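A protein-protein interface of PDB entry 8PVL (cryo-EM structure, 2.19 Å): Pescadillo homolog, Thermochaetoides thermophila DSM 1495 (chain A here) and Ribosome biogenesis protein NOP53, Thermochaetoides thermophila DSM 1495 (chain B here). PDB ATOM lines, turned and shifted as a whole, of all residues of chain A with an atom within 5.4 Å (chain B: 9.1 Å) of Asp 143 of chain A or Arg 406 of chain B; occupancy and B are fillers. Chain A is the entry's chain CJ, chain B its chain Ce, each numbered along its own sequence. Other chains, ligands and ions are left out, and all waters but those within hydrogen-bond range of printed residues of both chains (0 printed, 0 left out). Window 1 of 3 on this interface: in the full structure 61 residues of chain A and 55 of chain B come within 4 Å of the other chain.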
ATOM      1  N   ASP A 140      -9.755  17.349   1.768  1.00  0.00           N
ATOM      2  CA  ASP A 140      -9.397  17.254   0.351  1.00  0.00           C
ATOM      3  C   ASP A 140      -9.457  18.598  -0.380  1.00  0.00           C
ATOM      4  O   ASP A 140      -9.091  18.679  -1.571  1.00  0.00           O
ATOM      5  CB  ASP A 140     -10.307  16.251  -0.353  1.00  0.00           C
ATOM      6  CG  ASP A 140      -9.534  15.206  -1.124  1.00  0.00           C
ATOM      7  OD1 ASP A 140      -8.483  14.755  -0.623  1.00  0.00           O
ATOM      8  OD2 ASP A 140      -9.974  14.834  -2.231  1.00  0.00           O
ATOM      9  N   LEU A 141      -9.924  19.643   0.308  1.00  0.00           N
ATOM     10  CA  LEU A 141     -10.031  20.968  -0.297  1.00  0.00           C
ATOM     11  C   LEU A 141      -8.706  21.531  -0.802  1.00  0.00           C
ATOM     12  O   LEU A 141      -8.730  22.365  -1.705  1.00  0.00           O
ATOM     13  CB  LEU A 141     -10.644  21.958   0.694  1.00  0.00           C
ATOM     14  CG  LEU A 141     -12.158  22.166   0.616  1.00  0.00           C
ATOM     15  CD1 LEU A 141     -12.546  23.456   1.309  1.00  0.00           C
ATOM     16  CD2 LEU A 141     -12.646  22.167  -0.824  1.00  0.00           C
ATOM     17  N   ASP A 142      -7.558  21.099  -0.270  1.00  0.00           N
ATOM     18  CA  ASP A 142      -6.278  21.618  -0.755  1.00  0.00           C
ATOM     19  C   ASP A 142      -6.043  21.243  -2.216  1.00  0.00           C
ATOM     20  O   ASP A 142      -5.793  22.113  -3.065  1.00  0.00           O
ATOM     21  CB  ASP A 142      -5.137  21.096   0.118  1.00  0.00           C
ATOM     22  CG  ASP A 142      -5.311  21.446   1.579  1.00  0.00           C
ATOM     23  OD1 ASP A 142      -6.460  21.698   2.000  1.00  0.00           O
ATOM     24  OD2 ASP A 142      -4.298  21.471   2.308  1.00  0.00           O
ATOM     25  N   ASP A 143      -6.157  19.948  -2.525  1.00  0.00           N
ATOM     26  CA  ASP A 143      -6.040  19.480  -3.901  1.00  0.00           C
ATOM     27  C   ASP A 143      -7.141  20.060  -4.777  1.00  0.00           C
ATOM     28  O   ASP A 143      -6.879  20.481  -5.915  1.00  0.00           O
ATOM     29  CB  ASP A 143      -6.084  17.954  -3.933  1.00  0.00           C
ATOM     30  CG  ASP A 143      -5.123  17.362  -4.939  1.00  0.00           C
ATOM     31  OD1 ASP A 143      -4.443  18.134  -5.645  1.00  0.00           O
ATOM     32  OD2 ASP A 143      -5.049  16.119  -5.027  1.00  0.00           O
ATOM     33  N   CYS A 144      -8.376  20.107  -4.253  1.00  0.00           N
ATOM     34  CA  CYS A 144      -9.495  20.626  -5.041  1.00  0.00           C
ATOM     35  C   CYS A 144      -9.276  22.085  -5.442  1.00  0.00           C
ATOM     36  O   CYS A 144      -9.433  22.452  -6.615  1.00  0.00           O
ATOM     37  CB  CYS A 144     -10.795  20.472  -4.252  1.00  0.00           C
ATOM     38  SG  CYS A 144     -12.200  21.378  -4.928  1.00  0.00           S
ATOM     39  N   LEU A 145      -8.870  22.923  -4.485  1.00  0.00           N
ATOM     40  CA  LEU A 145      -8.703  24.344  -4.756  1.00  0.00           C
ATOM     41  C   LEU A 145      -7.489  24.609  -5.629  1.00  0.00           C
ATOM     42  O   LEU A 145      -7.533  25.496  -6.487  1.00  0.00           O
ATOM     43  CB  LEU A 145      -8.597  25.124  -3.448  1.00  0.00           C
ATOM     44  CG  LEU A 145      -9.880  25.244  -2.629  1.00  0.00           C
ATOM     45  CD1 LEU A 145      -9.539  25.556  -1.188  1.00  0.00           C
ATOM     46  CD2 LEU A 145     -10.791  26.300  -3.218  1.00  0.00           C
ATOM     47  N   SER A 146      -6.398  23.856  -5.434  1.00  0.00           N
ATOM     48  CA  SER A 146      -5.236  24.031  -6.301  1.00  0.00           C
ATOM     49  C   SER A 146      -5.577  23.707  -7.751  1.00  0.00           C
ATOM     50  O   SER A 146      -5.258  24.489  -8.659  1.00  0.00           O
ATOM     51  CB  SER A 146      -4.078  23.163  -5.815  1.00  0.00           C
ATOM     52  OG  SER A 146      -3.576  23.639  -4.581  1.00  0.00           O
ATOM     53  N   MET A 147      -6.289  22.595  -7.978  1.00  0.00           N
ATOM     54  CA  MET A 147      -6.665  22.224  -9.340  1.00  0.00           C
ATOM     55  C   MET A 147      -7.619  23.242  -9.963  1.00  0.00           C
ATOM     56  O   MET A 147      -7.435  23.644 -11.120  1.00  0.00           O
ATOM     57  CB  MET A 147      -7.293  20.832  -9.347  1.00  0.00           C
ATOM     58  CG  MET A 147      -6.291  19.712  -9.542  1.00  0.00           C
ATOM     59  SD  MET A 147      -5.523  19.769 -11.169  1.00  0.00           S
ATOM     60  CE  MET A 147      -6.652  18.749 -12.104  1.00  0.00           C
ATOM     61  N   LEU A 148      -8.628  23.690  -9.210  1.00  0.00           N
ATOM     62  CA  LEU A 148      -9.623  24.580  -9.803  1.00  0.00           C
ATOM     63  C   LEU A 148      -9.066  25.982 -10.032  1.00  0.00           C
ATOM     64  O   LEU A 148      -9.374  26.617 -11.050  1.00  0.00           O
ATOM     65  CB  LEU A 148     -10.877  24.624  -8.933  1.00  0.00           C
ATOM     66  CG  LEU A 148     -11.701  23.333  -8.936  1.00  0.00           C
ATOM     67  CD1 LEU A 148     -13.054  23.558  -8.306  1.00  0.00           C
ATOM     68  CD2 LEU A 148     -11.858  22.768 -10.340  1.00  0.00           C
ATOM     69  N   LEU A 150      -5.954  26.592 -10.669  1.00  0.00           N
ATOM     70  CA  LEU A 150      -5.105  26.451 -11.844  1.00  0.00           C
ATOM     71  C   LEU A 150      -5.928  26.477 -13.127  1.00  0.00           C
ATOM     72  O   LEU A 150      -5.587  27.185 -14.081  1.00  0.00           O
ATOM     73  CB  LEU A 150      -4.303  25.158 -11.744  1.00  0.00           C
ATOM     74  CG  LEU A 150      -3.577  24.670 -12.992  1.00  0.00           C
ATOM     75  CD1 LEU A 150      -2.476  25.629 -13.413  1.00  0.00           C
ATOM     76  CD2 LEU A 150      -3.026  23.297 -12.714  1.00  0.00           C
ATOM     77  N   LEU A 209      -2.376  26.580  -3.626  1.00  0.00           N
ATOM     78  CA  LEU A 209      -1.431  27.358  -4.415  1.00  0.00           C
ATOM     79  C   LEU A 209      -2.108  27.852  -5.687  1.00  0.00           C
ATOM     80  O   LEU A 209      -2.738  27.069  -6.404  1.00  0.00           O
ATOM     81  CB  LEU A 209      -0.200  26.512  -4.749  1.00  0.00           C
ATOM     82  CG  LEU A 209       0.871  27.042  -5.701  1.00  0.00           C
ATOM     83  CD1 LEU A 209       1.484  28.322  -5.178  1.00  0.00           C
ATOM     84  CD2 LEU A 209       1.939  25.983  -5.900  1.00  0.00           C
ATOM     85  N   MET A 227      -6.510  15.038 -16.383  1.00  0.00           N
ATOM     86  CA  MET A 227      -6.597  16.247 -15.569  1.00  0.00           C
ATOM     87  C   MET A 227      -7.983  16.874 -15.672  1.00  0.00           C
ATOM     88  O   MET A 227      -8.516  17.387 -14.685  1.00  0.00           O
ATOM     89  CB  MET A 227      -5.529  17.256 -15.994  1.00  0.00           C
ATOM     90  CG  MET A 227      -4.073  16.859 -15.739  1.00  0.00           C
ATOM     91  SD  MET A 227      -3.470  16.930 -14.040  1.00  0.00           S
ATOM     92  CE  MET A 227      -3.763  15.253 -13.491  1.00  0.00           C
ATOM     93  N   TYR A 234     -13.616  17.737  -9.058  1.00  0.00           N
ATOM     94  CA  TYR A 234     -13.358  18.749  -8.040  1.00  0.00           C
ATOM     95  C   TYR A 234     -14.343  19.907  -8.119  1.00  0.00           C
ATOM     96  O   TYR A 234     -14.693  20.485  -7.086  1.00  0.00           O
ATOM     97  CB  TYR A 234     -11.922  19.250  -8.154  1.00  0.00           C
ATOM     98  CG  TYR A 234     -10.926  18.297  -7.546  1.00  0.00           C
ATOM     99  CD1 TYR A 234     -11.233  17.595  -6.388  1.00  0.00           C
ATOM    100  CD2 TYR A 234      -9.686  18.088  -8.131  1.00  0.00           C
ATOM    101  CE1 TYR A 234     -10.331  16.717  -5.827  1.00  0.00           C
ATOM    102  CE2 TYR A 234      -8.776  17.211  -7.577  1.00  0.00           C
ATOM    103  CZ  TYR A 234      -9.105  16.530  -6.426  1.00  0.00           C
ATOM    104  OH  TYR A 234      -8.205  15.655  -5.868  1.00  0.00           O
ATOM    105  N   VAL B 203       2.750  11.608   0.911  1.00  0.00           N
ATOM    106  CA  VAL B 203       3.146  12.963   0.535  1.00  0.00           C
ATOM    107  C   VAL B 203       1.918  13.863   0.590  1.00  0.00           C
ATOM    108  O   VAL B 203       0.840  13.457   0.134  1.00  0.00           O
ATOM    109  CB  VAL B 203       3.792  12.973  -0.861  1.00  0.00           C
ATOM    110  CG1 VAL B 203       4.218  14.374  -1.269  1.00  0.00           C
ATOM    111  CG2 VAL B 203       4.974  12.020  -0.901  1.00  0.00           C
ATOM    112  N   PRO B 204       2.016  15.066   1.161  1.00  0.00           N
ATOM    113  CA  PRO B 204       0.889  16.006   1.095  1.00  0.00           C
ATOM    114  C   PRO B 204       0.619  16.454  -0.334  1.00  0.00           C
ATOM    115  O   PRO B 204       1.518  16.486  -1.178  1.00  0.00           O
ATOM    116  CB  PRO B 204       1.350  17.180   1.968  1.00  0.00           C
ATOM    117  CG  PRO B 204       2.457  16.641   2.799  1.00  0.00           C
ATOM    118  CD  PRO B 204       3.119  15.586   1.984  1.00  0.00           C
ATOM    119  N   ALA B 205      -0.649  16.782  -0.602  1.00  0.00           N
ATOM    120  CA  ALA B 205      -1.036  17.252  -1.929  1.00  0.00           C
ATOM    121  C   ALA B 205      -0.366  18.577  -2.265  1.00  0.00           C
ATOM    122  O   ALA B 205       0.113  18.773  -3.387  1.00  0.00           O
ATOM    123  CB  ALA B 205      -2.556  17.384  -2.015  1.00  0.00           C
ATOM    124  N   VAL B 206      -0.329  19.497  -1.310  1.00  0.00           N
ATOM    125  CA  VAL B 206       0.412  20.743  -1.429  1.00  0.00           C
ATOM    126  C   VAL B 206       1.408  20.810  -0.278  1.00  0.00           C
ATOM    127  O   VAL B 206       1.032  21.068   0.866  1.00  0.00           O
ATOM    128  CB  VAL B 206      -0.522  21.966  -1.425  1.00  0.00           C
ATOM    129  CG1 VAL B 206       0.281  23.240  -1.624  1.00  0.00           C
ATOM    130  CG2 VAL B 206      -1.585  21.838  -2.503  1.00  0.00           C
ATOM    131  N   PRO B 207       2.687  20.550  -0.537  1.00  0.00           N
ATOM    132  CA  PRO B 207       3.692  20.654   0.526  1.00  0.00           C
ATOM    133  C   PRO B 207       3.890  22.092   0.976  1.00  0.00           C
ATOM    134  O   PRO B 207       3.688  23.042   0.216  1.00  0.00           O
ATOM    135  CB  PRO B 207       4.962  20.097  -0.129  1.00  0.00           C
ATOM    136  CG  PRO B 207       4.472  19.284  -1.286  1.00  0.00           C
ATOM    137  CD  PRO B 207       3.260  20.003  -1.778  1.00  0.00           C
ATOM    138  N   ASP B 363       8.541  14.281  -1.679  1.00  0.00           N
ATOM    139  CA  ASP B 363       8.373  14.039  -3.106  1.00  0.00           C
ATOM    140  C   ASP B 363       9.645  14.281  -3.908  1.00  0.00           C
ATOM    141  O   ASP B 363       9.673  13.958  -5.100  1.00  0.00           O
ATOM    142  CB  ASP B 363       7.239  14.906  -3.664  1.00  0.00           C
ATOM    143  CG  ASP B 363       7.226  16.305  -3.077  1.00  0.00           C
ATOM    144  OD1 ASP B 363       7.763  16.497  -1.967  1.00  0.00           O
ATOM    145  OD2 ASP B 363       6.674  17.215  -3.730  1.00  0.00           O
ATOM    146  N   LEU B 376       9.548   8.264 -12.618  1.00  0.00           N
ATOM    147  CA  LEU B 376       9.396   9.704 -12.755  1.00  0.00           C
ATOM    148  C   LEU B 376      10.764  10.382 -12.788  1.00  0.00           C
ATOM    149  O   LEU B 376      11.656  10.020 -12.017  1.00  0.00           O
ATOM    150  CB  LEU B 376       8.570  10.273 -11.605  1.00  0.00           C
ATOM    151  CG  LEU B 376       7.051  10.260 -11.752  1.00  0.00           C
ATOM    152  CD1 LEU B 376       6.422  10.943 -10.557  1.00  0.00           C
ATOM    153  CD2 LEU B 376       6.627  10.936 -13.041  1.00  0.00           C
ATOM    154  N   ASN B 401       6.127  24.568 -13.489  1.00  0.00           N
ATOM    155  CA  ASN B 401       4.858  24.441 -14.195  1.00  0.00           C
ATOM    156  C   ASN B 401       3.861  23.817 -13.235  1.00  0.00           C
ATOM    157  O   ASN B 401       4.065  22.687 -12.783  1.00  0.00           O
ATOM    158  CB  ASN B 401       5.014  23.591 -15.458  1.00  0.00           C
ATOM    159  CG  ASN B 401       3.836  23.718 -16.396  1.00  0.00           C
ATOM    160  OD1 ASN B 401       2.730  23.284 -16.087  1.00  0.00           O
ATOM    161  ND2 ASN B 401       4.071  24.315 -17.557  1.00  0.00           N
ATOM    162  N   LEU B 402       2.793  24.549 -12.919  1.00  0.00           N
ATOM    163  CA  LEU B 402       1.872  24.096 -11.883  1.00  0.00           C
ATOM    164  C   LEU B 402       1.009  22.931 -12.352  1.00  0.00           C
ATOM    165  O   LEU B 402       0.656  22.067 -11.543  1.00  0.00           O
ATOM    166  CB  LEU B 402       1.002  25.259 -11.409  1.00  0.00           C
ATOM    167  CG  LEU B 402       1.736  26.354 -10.629  1.00  0.00           C
ATOM    168  CD1 LEU B 402       0.749  27.237  -9.894  1.00  0.00           C
ATOM    169  CD2 LEU B 402       2.748  25.770  -9.655  1.00  0.00           C
ATOM    170  N   LEU B 403       0.663  22.886 -13.640  1.00  0.00           N
ATOM    171  CA  LEU B 403      -0.066  21.738 -14.175  1.00  0.00           C
ATOM    172  C   LEU B 403       0.778  20.473 -14.108  1.00  0.00           C
ATOM    173  O   LEU B 403       0.289  19.404 -13.712  1.00  0.00           O
ATOM    174  CB  LEU B 403      -0.502  22.030 -15.611  1.00  0.00           C
ATOM    175  CG  LEU B 403      -1.418  21.019 -16.300  1.00  0.00           C
ATOM    176  CD1 LEU B 403      -2.700  20.829 -15.514  1.00  0.00           C
ATOM    177  CD2 LEU B 403      -1.726  21.471 -17.716  1.00  0.00           C
ATOM    178  N   LYS B 404       2.059  20.590 -14.466  1.00  0.00           N
ATOM    179  CA  LYS B 404       2.990  19.479 -14.319  1.00  0.00           C
ATOM    180  C   LYS B 404       3.169  19.096 -12.860  1.00  0.00           C
ATOM    181  O   LYS B 404       3.318  17.911 -12.546  1.00  0.00           O
ATOM    182  CB  LYS B 404       4.332  19.843 -14.950  1.00  0.00           C
ATOM    183  CG  LYS B 404       5.236  18.663 -15.230  1.00  0.00           C
ATOM    184  CD  LYS B 404       6.481  19.101 -15.977  1.00  0.00           C
ATOM    185  CE  LYS B 404       7.351  17.914 -16.349  1.00  0.00           C
ATOM    186  NZ  LYS B 404       8.604  18.343 -17.027  1.00  0.00           N
ATOM    187  N   ASP B 405       3.142  20.081 -11.958  1.00  0.00           N
ATOM    188  CA  ASP B 405       3.257  19.798 -10.533  1.00  0.00           C
ATOM    189  C   ASP B 405       2.054  19.020 -10.016  1.00  0.00           C
ATOM    190  O   ASP B 405       2.213  18.092  -9.221  1.00  0.00           O
ATOM    191  CB  ASP B 405       3.430  21.100  -9.753  1.00  0.00           C
ATOM    192  CG  ASP B 405       4.882  21.476  -9.568  1.00  0.00           C
ATOM    193  OD1 ASP B 405       5.716  20.562  -9.405  1.00  0.00           O
ATOM    194  OD2 ASP B 405       5.190  22.685  -9.587  1.00  0.00           O
ATOM    195  N   ARG B 406       0.845  19.386 -10.451  1.00  0.00           N
ATOM    196  CA  ARG B 406      -0.347  18.646 -10.037  1.00  0.00           C
ATOM    197  C   ARG B 406      -0.343  17.226 -10.592  1.00  0.00           C
ATOM    198  O   ARG B 406      -0.713  16.275  -9.887  1.00  0.00           O
ATOM    199  CB  ARG B 406      -1.614  19.383 -10.471  1.00  0.00           C
ATOM    200  CG  ARG B 406      -1.788  20.767  -9.870  1.00  0.00           C
ATOM    201  CD  ARG B 406      -2.665  20.762  -8.622  1.00  0.00           C
ATOM    202  NE  ARG B 406      -2.136  19.929  -7.549  1.00  0.00           N
ATOM    203  CZ  ARG B 406      -1.127  20.267  -6.758  1.00  0.00           C
ATOM    204  NH1 ARG B 406      -0.502  21.425  -6.888  1.00  0.00           N
ATOM    205  NH2 ARG B 406      -0.736  19.421  -5.810  1.00  0.00           N
ATOM    206  N   TYR B 407       0.076  17.066 -11.852  1.00  0.00           N
ATOM    207  CA  TYR B 407       0.167  15.735 -12.446  1.00  0.00           C
ATOM    208  C   TYR B 407       1.191  14.866 -11.716  1.00  0.00           C
ATOM    209  O   TYR B 407       0.921  13.695 -11.406  1.00  0.00           O
ATOM    210  CB  TYR B 407       0.511  15.869 -13.928  1.00  0.00           C
ATOM    211  CG  TYR B 407       0.560  14.571 -14.689  1.00  0.00           C
ATOM    212  CD1 TYR B 407      -0.551  13.744 -14.760  1.00  0.00           C
ATOM    213  CD2 TYR B 407       1.713  14.181 -15.355  1.00  0.00           C
ATOM    214  CE1 TYR B 407      -0.513  12.559 -15.461  1.00  0.00           C
ATOM    215  CE2 TYR B 407       1.760  13.000 -16.063  1.00  0.00           C
ATOM    216  CZ  TYR B 407       0.645  12.192 -16.111  1.00  0.00           C
ATOM    217  OH  TYR B 407       0.683  11.010 -16.811  1.00  0.00           O
ATOM    218  N   ARG B 408       2.357  15.440 -11.400  1.00  0.00           N
ATOM    219  CA  ARG B 408       3.377  14.723 -10.640  1.00  0.00           C
ATOM    220  C   ARG B 408       2.899  14.394  -9.235  1.00  0.00           C
ATOM    221  O   ARG B 408       3.212  13.325  -8.706  1.00  0.00           O
ATOM    222  CB  ARG B 408       4.665  15.541 -10.574  1.00  0.00           C
ATOM    223  CG  ARG B 408       5.728  15.119 -11.565  1.00  0.00           C
ATOM    224  CD  ARG B 408       7.055  15.788 -11.251  1.00  0.00           C
ATOM    225  NE  ARG B 408       7.536  15.449  -9.917  1.00  0.00           N
ATOM    226  CZ  ARG B 408       8.578  14.666  -9.673  1.00  0.00           C
ATOM    227  NH1 ARG B 408       9.271  14.112 -10.653  1.00  0.00           N
ATOM    228  NH2 ARG B 408       8.932  14.433  -8.414  1.00  0.00           N
ATOM    229  N   SER B 409       2.158  15.312  -8.607  1.00  0.00           N
ATOM    230  CA  SER B 409       1.647  15.077  -7.263  1.00  0.00           C
ATOM    231  C   SER B 409       0.662  13.919  -7.243  1.00  0.00           C
ATOM    232  O   SER B 409       0.703  13.078  -6.339  1.00  0.00           O
ATOM    233  CB  SER B 409       0.991  16.346  -6.724  1.00  0.00           C
ATOM    234  OG  SER B 409       0.390  16.117  -5.465  1.00  0.00           O
ATOM    235  N   MET B 410      -0.217  13.848  -8.244  1.00  0.00           N
ATOM    236  CA  MET B 410      -1.160  12.736  -8.305  1.00  0.00           C
ATOM    237  C   MET B 410      -0.455  11.412  -8.589  1.00  0.00           C
ATOM    238  O   MET B 410      -0.812  10.379  -8.004  1.00  0.00           O
ATOM    239  CB  MET B 410      -2.243  13.029  -9.339  1.00  0.00           C
ATOM    240  CG  MET B 410      -3.417  13.799  -8.755  1.00  0.00           C
ATOM    241  SD  MET B 410      -4.200  14.934  -9.909  1.00  0.00           S
ATOM    242  CE  MET B 410      -5.243  15.870  -8.796  1.00  0.00           C
ATOM    243  N   ILE B 411       0.562  11.419  -9.461  1.00  0.00           N
ATOM    244  CA  ILE B 411       1.315  10.190  -9.716  1.00  0.00           C
ATOM    245  C   ILE B 411       2.067   9.738  -8.465  1.00  0.00           C
ATOM    246  O   ILE B 411       2.066   8.549  -8.122  1.00  0.00           O
ATOM    247  CB  ILE B 411       2.266  10.373 -10.913  1.00  0.00           C
ATOM    248  CG1 ILE B 411       1.474  10.544 -12.207  1.00  0.00           C
ATOM    249  CG2 ILE B 411       3.202   9.178 -11.053  1.00  0.00           C
ATOM    250  CD1 ILE B 411       2.348  10.689 -13.420  1.00  0.00           C
ATOM    251  N   VAL B 412       2.703  10.677  -7.757  1.00  0.00           N
ATOM    252  CA  VAL B 412       3.480  10.347  -6.564  1.00  0.00           C
ATOM    253  C   VAL B 412       2.571   9.848  -5.446  1.00  0.00           C
ATOM    254  O   VAL B 412       2.881   8.858  -4.773  1.00  0.00           O
ATOM    255  CB  VAL B 412       4.317  11.568  -6.132  1.00  0.00           C
ATOM    256  CG1 VAL B 412       4.718  11.483  -4.668  1.00  0.00           C
ATOM    257  CG2 VAL B 412       5.554  11.690  -7.001  1.00  0.00           C
ATOM    258  N   ARG B 413       1.422  10.492  -5.253  1.00  0.00           N
ATOM    259  CA  ARG B 413       0.479  10.045  -4.240  1.00  0.00           C
ATOM    260  C   ARG B 413      -0.302   8.808  -4.660  1.00  0.00           C
ATOM    261  O   ARG B 413      -1.038   8.254  -3.839  1.00  0.00           O
ATOM    262  CB  ARG B 413      -0.480  11.180  -3.884  1.00  0.00           C
ATOM    263  CG  ARG B 413       0.191  12.311  -3.124  1.00  0.00           C
ATOM    264  CD  ARG B 413      -0.795  13.400  -2.765  1.00  0.00           C
ATOM    265  NE  ARG B 413      -1.186  14.173  -3.935  1.00  0.00           N
ATOM    266  CZ  ARG B 413      -2.426  14.565  -4.189  1.00  0.00           C
ATOM    267  NH1 ARG B 413      -3.424  14.273  -3.371  1.00  0.00           N
ATOM    268  NH2 ARG B 413      -2.670  15.267  -5.290  1.00  0.00           N
ATOM    269  N   GLY B 414      -0.175   8.371  -5.910  1.00  0.00           N
ATOM    270  CA  GLY B 414      -0.619   7.043  -6.279  1.00  0.00           C
ATOM    271  C   GLY B 414      -2.047   6.938  -6.746  1.00  0.00           C
ATOM    272  O   GLY B 414      -2.587   5.826  -6.789  1.00  0.00           O
ATOM    273  N   LYS B 415      -2.682   8.056  -7.093  1.00  0.00           N
ATOM    274  CA  LYS B 415      -4.037   8.006  -7.622  1.00  0.00           C
ATOM    275  C   LYS B 415      -4.076   7.458  -9.041  1.00  0.00           C
ATOM    276  O   LYS B 415      -5.124   6.972  -9.475  1.00  0.00           O
ATOM    277  CB  LYS B 415      -4.661   9.398  -7.566  1.00  0.00           C
ATOM    278  CG  LYS B 415      -4.758   9.951  -6.157  1.00  0.00           C
ATOM    279  CD  LYS B 415      -5.353  11.344  -6.139  1.00  0.00           C
ATOM    280  CE  LYS B 415      -5.607  11.808  -4.716  1.00  0.00           C
ATOM    281  NZ  LYS B 415      -6.215  13.165  -4.678  1.00  0.00           N
ATOM    282  N   LEU B 416      -2.958   7.518  -9.759  1.00  0.00           N
ATOM    283  CA  LEU B 416      -2.857   6.975 -11.107  1.00  0.00           C
ATOM    284  C   LEU B 416      -1.387   6.718 -11.407  1.00  0.00           C
ATOM    285  O   LEU B 416      -0.496   7.192 -10.698  1.00  0.00           O
ATOM    286  CB  LEU B 416      -3.484   7.913 -12.147  1.00  0.00           C
ATOM    287  CG  LEU B 416      -2.665   9.072 -12.719  1.00  0.00           C
ATOM    288  CD1 LEU B 416      -3.360   9.622 -13.947  1.00  0.00           C
ATOM    289  CD2 LEU B 416      -2.464  10.175 -11.700  1.00  0.00           C
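Hydrophobic or aromatic side chains of chain B within 4 Å of the printed part of chain A: Ala 205, Val 206, Leu 402, Leu 403, Tyr 407 and Met 410.
Of the 13 printed residues of chain A, 7 touch a printed residue of chain B.
Printed residues of chain A that touch a printed residue of chain B: Asp 143, Ser 146, Met 147, Leu 150, Leu 209, Met 227 and Tyr 234.
Hydrophobic or aromatic side chains of chain A within 4 Å of the printed part of chain B: Met 147, Leu 150, Leu 209, Met 227 and Tyr 234.
The guanidinium group (NH2) of Arg 413 of chain B is in salt-bridge range of the side-chain carboxylate (OD2) of Asp 143 of chain A, at 2.5 Å.
NZ of Lys 415 of chain B lies within hydrogen-bond range of OH of Tyr 234 of chain A (3.4 Å).
The guanidinium group of Arg 406 of chain B lies within salt-bridge range of the side-chain carboxylate of Asp 143 of chain A, 3.5 Å away.
NZ of Lys 415 of chain B is in salt-bridge range of OD2 of Asp 143 of chain A (3.2 Å).
Among the printed residues, merely in contact across the chains: Ser 146 of chain A with Val 206 of chain B (3.4 Å), Met 227 of chain A with Met 410 of chain B (3.6 Å), Leu 150 of chain A with Leu 403 of chain B (3.7 Å), Met 227 of chain A with Tyr 407 of chain B (3.8 Å), Asp 143 of chain A with Met 410 of chain B (3.8 Å), Leu 209 of chain A with Leu 402 of chain B (3.8 Å), Met 147 of chain A with Arg 406 of chain B (3.9 Å), Asp 143 of chain A with Ala 205 of chain B (3.9 Å), Ser 146 of chain A with Arg 406 of chain B (3.95 Å) and Tyr 234 of chain A with Met 410 of chain B (3.97 Å).
The guanidinium group (NE) of Arg 413 of chain B lies within hydrogen-bond range of the side-chain hydroxyl (OG) of Ser 409 of chain B, 2.9 Å away.
The backbone carbonyl oxygen of Met 410 of chain B lies within hydrogen-bond range of the backbone NH of Lys 415 of chain B (3.1 Å).
The side-chain hydroxyl (OG) of Ser 146 of chain A is in hydrogen-bond range of the backbone NH (N) of Leu 209 of chain A, 3.3 Å away.
The side-chain sulfur (SG) of Cys 144 of chain A sits at hydrogen-bond distance from the backbone carbonyl oxygen (O) of Tyr 234 of chain A (3.4 Å).
The backbone carbonyl oxygen (O) of Ala 205 of chain B lies within hydrogen-bond range of the guanidinium group (NH2) of Arg 406 of chain B, 2.6 Å away.
The side-chain hydroxyl of Ser 146 of chain A lies within hydrogen-bond range of the backbone carbonyl oxygen of Asp 142 of chain A.
Leu 141 of chain A touches none of the printed residues of chain B.
Ser 146 of chain A touches just these residues of chain B: Val 206 and Arg 406.
Of the printed residues of chain B, Leu 150 of chain A touches Leu 403 (3.7 Å).
Printed residues of chain B within 4 Å of Leu 209 of chain A: Leu 402 (3.8 Å).
Of the printed residues of chain A, Leu 403 of chain B touches Leu 150 (3.7 Å).
Printed residues of chain A within 4 Å of Arg 406 of chain B: Asp 143 (3.5 Å), Ser 146 (3.95 Å) and Met 147 (3.9 Å).
The nearest residue of chain B that does not touch Asp 143 of chain A is Val 206 of chain B (4.9 Å).
The nearest printed residue of chain B that does not touch Leu 209 of chain A is Val 206 of chain B (4.6 Å).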
